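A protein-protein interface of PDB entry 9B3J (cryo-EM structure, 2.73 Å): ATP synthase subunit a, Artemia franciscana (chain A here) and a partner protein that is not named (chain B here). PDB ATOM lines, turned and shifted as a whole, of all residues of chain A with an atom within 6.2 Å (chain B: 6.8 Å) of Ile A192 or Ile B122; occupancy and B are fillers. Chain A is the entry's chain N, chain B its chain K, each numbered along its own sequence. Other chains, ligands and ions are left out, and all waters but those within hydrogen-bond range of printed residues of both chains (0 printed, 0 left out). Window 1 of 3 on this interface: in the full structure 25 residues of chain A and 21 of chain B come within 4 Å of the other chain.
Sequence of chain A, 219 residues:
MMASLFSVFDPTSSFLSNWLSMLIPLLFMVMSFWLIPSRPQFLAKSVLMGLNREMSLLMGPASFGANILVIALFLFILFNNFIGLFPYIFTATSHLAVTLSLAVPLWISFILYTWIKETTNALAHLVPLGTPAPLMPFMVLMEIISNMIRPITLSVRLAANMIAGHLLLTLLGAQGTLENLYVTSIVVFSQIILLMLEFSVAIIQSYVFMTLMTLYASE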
ATOM      1  N   VAL A 187       0.469  23.368   6.235  1.00  0.00           N
ATOM      2  CA  VAL A 187       1.571  23.933   7.006  1.00  0.00           C
ATOM      3  C   VAL A 187       1.546  23.418   8.438  1.00  0.00           C
ATOM      4  O   VAL A 187       2.579  23.012   8.975  1.00  0.00           O
ATOM      5  CB  VAL A 187       1.516  25.469   6.948  1.00  0.00           C
ATOM      6  CG1 VAL A 187       2.276  26.080   8.098  1.00  0.00           C
ATOM      7  CG2 VAL A 187       2.081  25.957   5.630  1.00  0.00           C
ATOM      8  N   VAL A 188       0.368  23.396   9.062  1.00  0.00           N
ATOM      9  CA  VAL A 188       0.248  22.929  10.441  1.00  0.00           C
ATOM     10  C   VAL A 188       0.580  21.442  10.544  1.00  0.00           C
ATOM     11  O   VAL A 188       1.265  21.015  11.482  1.00  0.00           O
ATOM     12  CB  VAL A 188      -1.154  23.253  10.987  1.00  0.00           C
ATOM     13  CG1 VAL A 188      -1.440  22.497  12.263  1.00  0.00           C
ATOM     14  CG2 VAL A 188      -1.268  24.727  11.245  1.00  0.00           C
ATOM     15  N   PHE A 189       0.134  20.632   9.578  1.00  0.00           N
ATOM     16  CA  PHE A 189       0.462  19.209   9.630  1.00  0.00           C
ATOM     17  C   PHE A 189       1.954  18.962   9.418  1.00  0.00           C
ATOM     18  O   PHE A 189       2.565  18.128  10.110  1.00  0.00           O
ATOM     19  CB  PHE A 189      -0.354  18.438   8.596  1.00  0.00           C
ATOM     20  CG  PHE A 189      -0.247  16.950   8.742  1.00  0.00           C
ATOM     21  CD1 PHE A 189      -0.986  16.285   9.705  1.00  0.00           C
ATOM     22  CD2 PHE A 189       0.601  16.216   7.930  1.00  0.00           C
ATOM     23  CE1 PHE A 189      -0.888  14.918   9.854  1.00  0.00           C
ATOM     24  CE2 PHE A 189       0.704  14.846   8.073  1.00  0.00           C
ATOM     25  CZ  PHE A 189      -0.042  14.198   9.036  1.00  0.00           C
ATOM     26  N   SER A 190       2.563  19.685   8.476  1.00  0.00           N
ATOM     27  CA  SER A 190       3.995  19.533   8.262  1.00  0.00           C
ATOM     28  C   SER A 190       4.793  20.064   9.442  1.00  0.00           C
ATOM     29  O   SER A 190       5.856  19.525   9.760  1.00  0.00           O
ATOM     30  CB  SER A 190       4.411  20.238   6.977  1.00  0.00           C
ATOM     31  OG  SER A 190       4.018  21.595   7.008  1.00  0.00           O
ATOM     32  N   GLN A 191       4.288  21.091  10.125  1.00  0.00           N
ATOM     33  CA  GLN A 191       4.976  21.584  11.308  1.00  0.00           C
ATOM     34  C   GLN A 191       4.796  20.653  12.492  1.00  0.00           C
ATOM     35  O   GLN A 191       5.644  20.632  13.377  1.00  0.00           O
ATOM     36  CB  GLN A 191       4.502  22.984  11.669  1.00  0.00           C
ATOM     37  CG  GLN A 191       5.117  24.048  10.811  1.00  0.00           C
ATOM     38  CD  GLN A 191       4.709  25.424  11.241  1.00  0.00           C
ATOM     39  OE1 GLN A 191       4.243  25.624  12.359  1.00  0.00           O
ATOM     40  NE2 GLN A 191       4.871  26.389  10.351  1.00  0.00           N
ATOM     41  N   ILE A 192       3.711  19.880  12.530  1.00  0.00           N
ATOM     42  CA  ILE A 192       3.571  18.866  13.572  1.00  0.00           C
ATOM     43  C   ILE A 192       4.598  17.757  13.377  1.00  0.00           C
ATOM     44  O   ILE A 192       5.251  17.316  14.338  1.00  0.00           O
ATOM     45  CB  ILE A 192       2.134  18.320  13.593  1.00  0.00           C
ATOM     46  CG1 ILE A 192       1.212  19.302  14.304  1.00  0.00           C
ATOM     47  CG2 ILE A 192       2.066  16.976  14.287  1.00  0.00           C
ATOM     48  CD1 ILE A 192      -0.221  18.895  14.264  1.00  0.00           C
ATOM     49  N   ILE A 193       4.781  17.316  12.128  1.00  0.00           N
ATOM     50  CA  ILE A 193       5.836  16.343  11.831  1.00  0.00           C
ATOM     51  C   ILE A 193       7.209  16.922  12.165  1.00  0.00           C
ATOM     52  O   ILE A 193       8.046  16.277  12.821  1.00  0.00           O
ATOM     53  CB  ILE A 193       5.755  15.903  10.361  1.00  0.00           C
ATOM     54  CG1 ILE A 193       4.494  15.077  10.127  1.00  0.00           C
ATOM     55  CG2 ILE A 193       6.989  15.121   9.963  1.00  0.00           C
ATOM     56  CD1 ILE A 193       4.366  14.557   8.715  1.00  0.00           C
ATOM     57  N   LEU A 194       7.443  18.167  11.755  1.00  0.00           N
ATOM     58  CA  LEU A 194       8.740  18.790  11.969  1.00  0.00           C
ATOM     59  C   LEU A 194       9.000  19.060  13.446  1.00  0.00           C
ATOM     60  O   LEU A 194      10.131  18.923  13.906  1.00  0.00           O
ATOM     61  CB  LEU A 194       8.830  20.075  11.154  1.00  0.00           C
ATOM     62  CG  LEU A 194      10.170  20.796  11.131  1.00  0.00           C
ATOM     63  CD1 LEU A 194      11.261  19.865  10.666  1.00  0.00           C
ATOM     64  CD2 LEU A 194      10.064  21.992  10.219  1.00  0.00           C
ATOM     65  N   LEU A 195       7.971  19.420  14.213  1.00  0.00           N
ATOM     66  CA  LEU A 195       8.173  19.707  15.627  1.00  0.00           C
ATOM     67  C   LEU A 195       8.380  18.441  16.437  1.00  0.00           C
ATOM     68  O   LEU A 195       9.105  18.469  17.438  1.00  0.00           O
ATOM     69  CB  LEU A 195       6.998  20.494  16.188  1.00  0.00           C
ATOM     70  CG  LEU A 195       7.097  22.004  16.052  1.00  0.00           C
ATOM     71  CD1 LEU A 195       5.723  22.589  16.141  1.00  0.00           C
ATOM     72  CD2 LEU A 195       7.978  22.567  17.142  1.00  0.00           C
ATOM     73  N   MET A 196       7.752  17.329  16.043  1.00  0.00           N
ATOM     74  CA  MET A 196       8.084  16.061  16.682  1.00  0.00           C
ATOM     75  C   MET A 196       9.530  15.678  16.405  1.00  0.00           C
ATOM     76  O   MET A 196      10.244  15.193  17.299  1.00  0.00           O
ATOM     77  CB  MET A 196       7.136  14.965  16.206  1.00  0.00           C
ATOM     78  CG  MET A 196       6.134  14.526  17.254  1.00  0.00           C
ATOM     79  SD  MET A 196       6.918  14.036  18.807  1.00  0.00           S
ATOM     80  CE  MET A 196       7.857  12.596  18.299  1.00  0.00           C
ATOM     81  N   LEU A 197       9.987  15.921  15.172  1.00  0.00           N
ATOM     82  CA  LEU A 197      11.392  15.696  14.854  1.00  0.00           C
ATOM     83  C   LEU A 197      12.300  16.621  15.656  1.00  0.00           C
ATOM     84  O   LEU A 197      13.365  16.203  16.117  1.00  0.00           O
ATOM     85  CB  LEU A 197      11.624  15.882  13.359  1.00  0.00           C
ATOM     86  CG  LEU A 197      13.066  15.926  12.867  1.00  0.00           C
ATOM     87  CD1 LEU A 197      13.768  14.631  13.171  1.00  0.00           C
ATOM     88  CD2 LEU A 197      13.090  16.201  11.384  1.00  0.00           C
ATOM     89  N   TYR B 115       1.600  29.703  13.933  1.00  0.00           N
ATOM     90  CA  TYR B 115       1.331  28.353  13.451  1.00  0.00           C
ATOM     91  C   TYR B 115       2.239  27.330  14.115  1.00  0.00           C
ATOM     92  O   TYR B 115       1.861  26.161  14.251  1.00  0.00           O
ATOM     93  CB  TYR B 115       1.477  28.310  11.937  1.00  0.00           C
ATOM     94  CG  TYR B 115       0.690  29.403  11.277  1.00  0.00           C
ATOM     95  CD1 TYR B 115      -0.687  29.317  11.167  1.00  0.00           C
ATOM     96  CD2 TYR B 115       1.316  30.534  10.792  1.00  0.00           C
ATOM     97  CE1 TYR B 115      -1.415  30.320  10.579  1.00  0.00           C
ATOM     98  CE2 TYR B 115       0.598  31.542  10.204  1.00  0.00           C
ATOM     99  CZ  TYR B 115      -0.767  31.431  10.098  1.00  0.00           C
ATOM    100  OH  TYR B 115      -1.481  32.440   9.504  1.00  0.00           O
ATOM    101  N   GLY B 117       2.951  27.727  17.322  1.00  0.00           N
ATOM    102  CA  GLY B 117       2.216  27.574  18.564  1.00  0.00           C
ATOM    103  C   GLY B 117       0.975  26.724  18.417  1.00  0.00           C
ATOM    104  O   GLY B 117       0.623  25.969  19.326  1.00  0.00           O
ATOM    105  N   VAL B 118       0.305  26.817  17.270  1.00  0.00           N
ATOM    106  CA  VAL B 118      -0.869  25.989  17.012  1.00  0.00           C
ATOM    107  C   VAL B 118      -0.472  24.523  16.893  1.00  0.00           C
ATOM    108  O   VAL B 118      -1.113  23.642  17.479  1.00  0.00           O
ATOM    109  CB  VAL B 118      -1.604  26.487  15.757  1.00  0.00           C
ATOM    110  CG1 VAL B 118      -2.553  25.432  15.225  1.00  0.00           C
ATOM    111  CG2 VAL B 118      -2.361  27.762  16.072  1.00  0.00           C
ATOM    112  N   ALA B 119       0.598  24.243  16.139  1.00  0.00           N
ATOM    113  CA  ALA B 119       1.052  22.867  15.968  1.00  0.00           C
ATOM    114  C   ALA B 119       1.537  22.272  17.282  1.00  0.00           C
ATOM    115  O   ALA B 119       1.336  21.080  17.545  1.00  0.00           O
ATOM    116  CB  ALA B 119       2.155  22.812  14.917  1.00  0.00           C
ATOM    117  N   ILE B 120       2.169  23.093  18.125  1.00  0.00           N
ATOM    118  CA  ILE B 120       2.554  22.650  19.461  1.00  0.00           C
ATOM    119  C   ILE B 120       1.322  22.352  20.301  1.00  0.00           C
ATOM    120  O   ILE B 120       1.292  21.368  21.041  1.00  0.00           O
ATOM    121  CB  ILE B 120       3.463  23.704  20.118  1.00  0.00           C
ATOM    122  CG1 ILE B 120       4.865  23.607  19.541  1.00  0.00           C
ATOM    123  CG2 ILE B 120       3.526  23.543  21.622  1.00  0.00           C
ATOM    124  CD1 ILE B 120       5.741  24.745  19.934  1.00  0.00           C
ATOM    125  N   ALA B 121       0.285  23.189  20.195  1.00  0.00           N
ATOM    126  CA  ALA B 121      -0.936  22.965  20.966  1.00  0.00           C
ATOM    127  C   ALA B 121      -1.642  21.682  20.547  1.00  0.00           C
ATOM    128  O   ALA B 121      -2.143  20.937  21.399  1.00  0.00           O
ATOM    129  CB  ALA B 121      -1.872  24.156  20.816  1.00  0.00           C
ATOM    130  N   ILE B 122      -1.683  21.405  19.244  1.00  0.00           N
ATOM    131  CA  ILE B 122      -2.302  20.170  18.765  1.00  0.00           C
ATOM    132  C   ILE B 122      -1.490  18.958  19.201  1.00  0.00           C
ATOM    133  O   ILE B 122      -2.045  17.963  19.691  1.00  0.00           O
ATOM    134  CB  ILE B 122      -2.486  20.214  17.239  1.00  0.00           C
ATOM    135  CG1 ILE B 122      -3.522  21.264  16.862  1.00  0.00           C
ATOM    136  CG2 ILE B 122      -2.939  18.877  16.725  1.00  0.00           C
ATOM    137  CD1 ILE B 122      -3.763  21.365  15.385  1.00  0.00           C
ATOM    138  N   MET B 123      -0.163  19.029  19.050  1.00  0.00           N
ATOM    139  CA  MET B 123       0.696  17.928  19.471  1.00  0.00           C
ATOM    140  C   MET B 123       0.624  17.708  20.973  1.00  0.00           C
ATOM    141  O   MET B 123       0.587  16.565  21.436  1.00  0.00           O
ATOM    142  CB  MET B 123       2.131  18.206  19.044  1.00  0.00           C
ATOM    143  CG  MET B 123       3.146  17.253  19.628  1.00  0.00           C
ATOM    144  SD  MET B 123       4.818  17.799  19.292  1.00  0.00           S
ATOM    145  CE  MET B 123       4.705  17.999  17.526  1.00  0.00           C
ATOM    146  N   GLY B 124       0.594  18.788  21.749  1.00  0.00           N
ATOM    147  CA  GLY B 124       0.521  18.658  23.189  1.00  0.00           C
ATOM    148  C   GLY B 124      -0.786  18.053  23.654  1.00  0.00           C
ATOM    149  O   GLY B 124      -0.796  17.212  24.555  1.00  0.00           O
ATOM    150  N   THR B 125      -1.902  18.456  23.036  1.00  0.00           N
ATOM    151  CA  THR B 125      -3.188  17.865  23.392  1.00  0.00           C
ATOM    152  C   THR B 125      -3.245  16.387  23.033  1.00  0.00           C
ATOM    153  O   THR B 125      -3.749  15.572  23.817  1.00  0.00           O
ATOM    154  CB  THR B 125      -4.316  18.618  22.701  1.00  0.00           C
ATOM    155  OG1 THR B 125      -3.962  18.840  21.333  1.00  0.00           O
ATOM    156  CG2 THR B 125      -4.556  19.946  23.376  1.00  0.00           C
ATOM    157  N   TYR B 126      -2.711  16.019  21.865  1.00  0.00           N
ATOM    158  CA  TYR B 126      -2.738  14.615  21.459  1.00  0.00           C
ATOM    159  C   TYR B 126      -1.816  13.763  22.326  1.00  0.00           C
ATOM    160  O   TYR B 126      -2.193  12.662  22.750  1.00  0.00           O
ATOM    161  CB  TYR B 126      -2.362  14.499  19.984  1.00  0.00           C
ATOM    162  CG  TYR B 126      -2.366  13.089  19.454  1.00  0.00           C
ATOM    163  CD1 TYR B 126      -3.556  12.445  19.151  1.00  0.00           C
ATOM    164  CD2 TYR B 126      -1.179  12.405  19.239  1.00  0.00           C
ATOM    165  CE1 TYR B 126      -3.563  11.151  18.658  1.00  0.00           C
ATOM    166  CE2 TYR B 126      -1.175  11.113  18.747  1.00  0.00           C
ATOM    167  CZ  TYR B 126      -2.369  10.492  18.458  1.00  0.00           C
ATOM    168  OH  TYR B 126      -2.367   9.208  17.968  1.00  0.00           O
ATOM    169  N   GLY B 127      -0.620  14.267  22.627  1.00  0.00           N
ATOM    170  CA  GLY B 127       0.306  13.516  23.455  1.00  0.00           C
ATOM    171  C   GLY B 127      -0.161  13.364  24.891  1.00  0.00           C
ATOM    172  O   GLY B 127      -0.006  12.295  25.486  1.00  0.00           O
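O of Tyr B115 lies close to OE1 of Gln A191 (3.1 Å).
O of Ile B122 sits at hydrogen-bond distance from OG1 of Thr B125, 2.7 Å away.
CB of Ala B119 touches O of Val A188, 3.98 Å away. Ile A192 touches Ala B119. CD1 of Ile A192 touches CG2 of Ile B122, at 3.7 Å. Ile A192 touches Met B123. CB of Ala B119 touches CD1 of Leu A195 (3.8 Å). Leu A195 touches Ile B120. Leu A195 touches Met B123. Met A196 touches Met B123.
Ile A192 touches just these residues of chain B: Ala B119, Ile B122 and Met B123. Ile B122 touches one residue of chain A. Of the printed residues of chain B, Leu A195 touches Ala B119, Ile B120 and Met B123. Printed residues of chain B within 4 Å of Gln A191: Tyr B115 (3.1 Å). Printed residues of chain A within 4 Å of Ala B119: Val A188 (3.98 Å), Ile A192 (3.7 Å) and Leu A195 (3.8 Å). The nearest residue of chain B that does not touch Ile A192 is Ile B120 (5.5 Å). The nearest residue of chain A that does not touch Ile B122 is Val A188 (4.1 Å). The nearest printed residue of chain A that does not touch Tyr B115 is Val A187 (4.5 Å).
Hydrophobic or aromatic side chains of chain B that line the printed part of chain A: Tyr B115, Ala B119, Ile B120, Ile B122 and Met B123.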
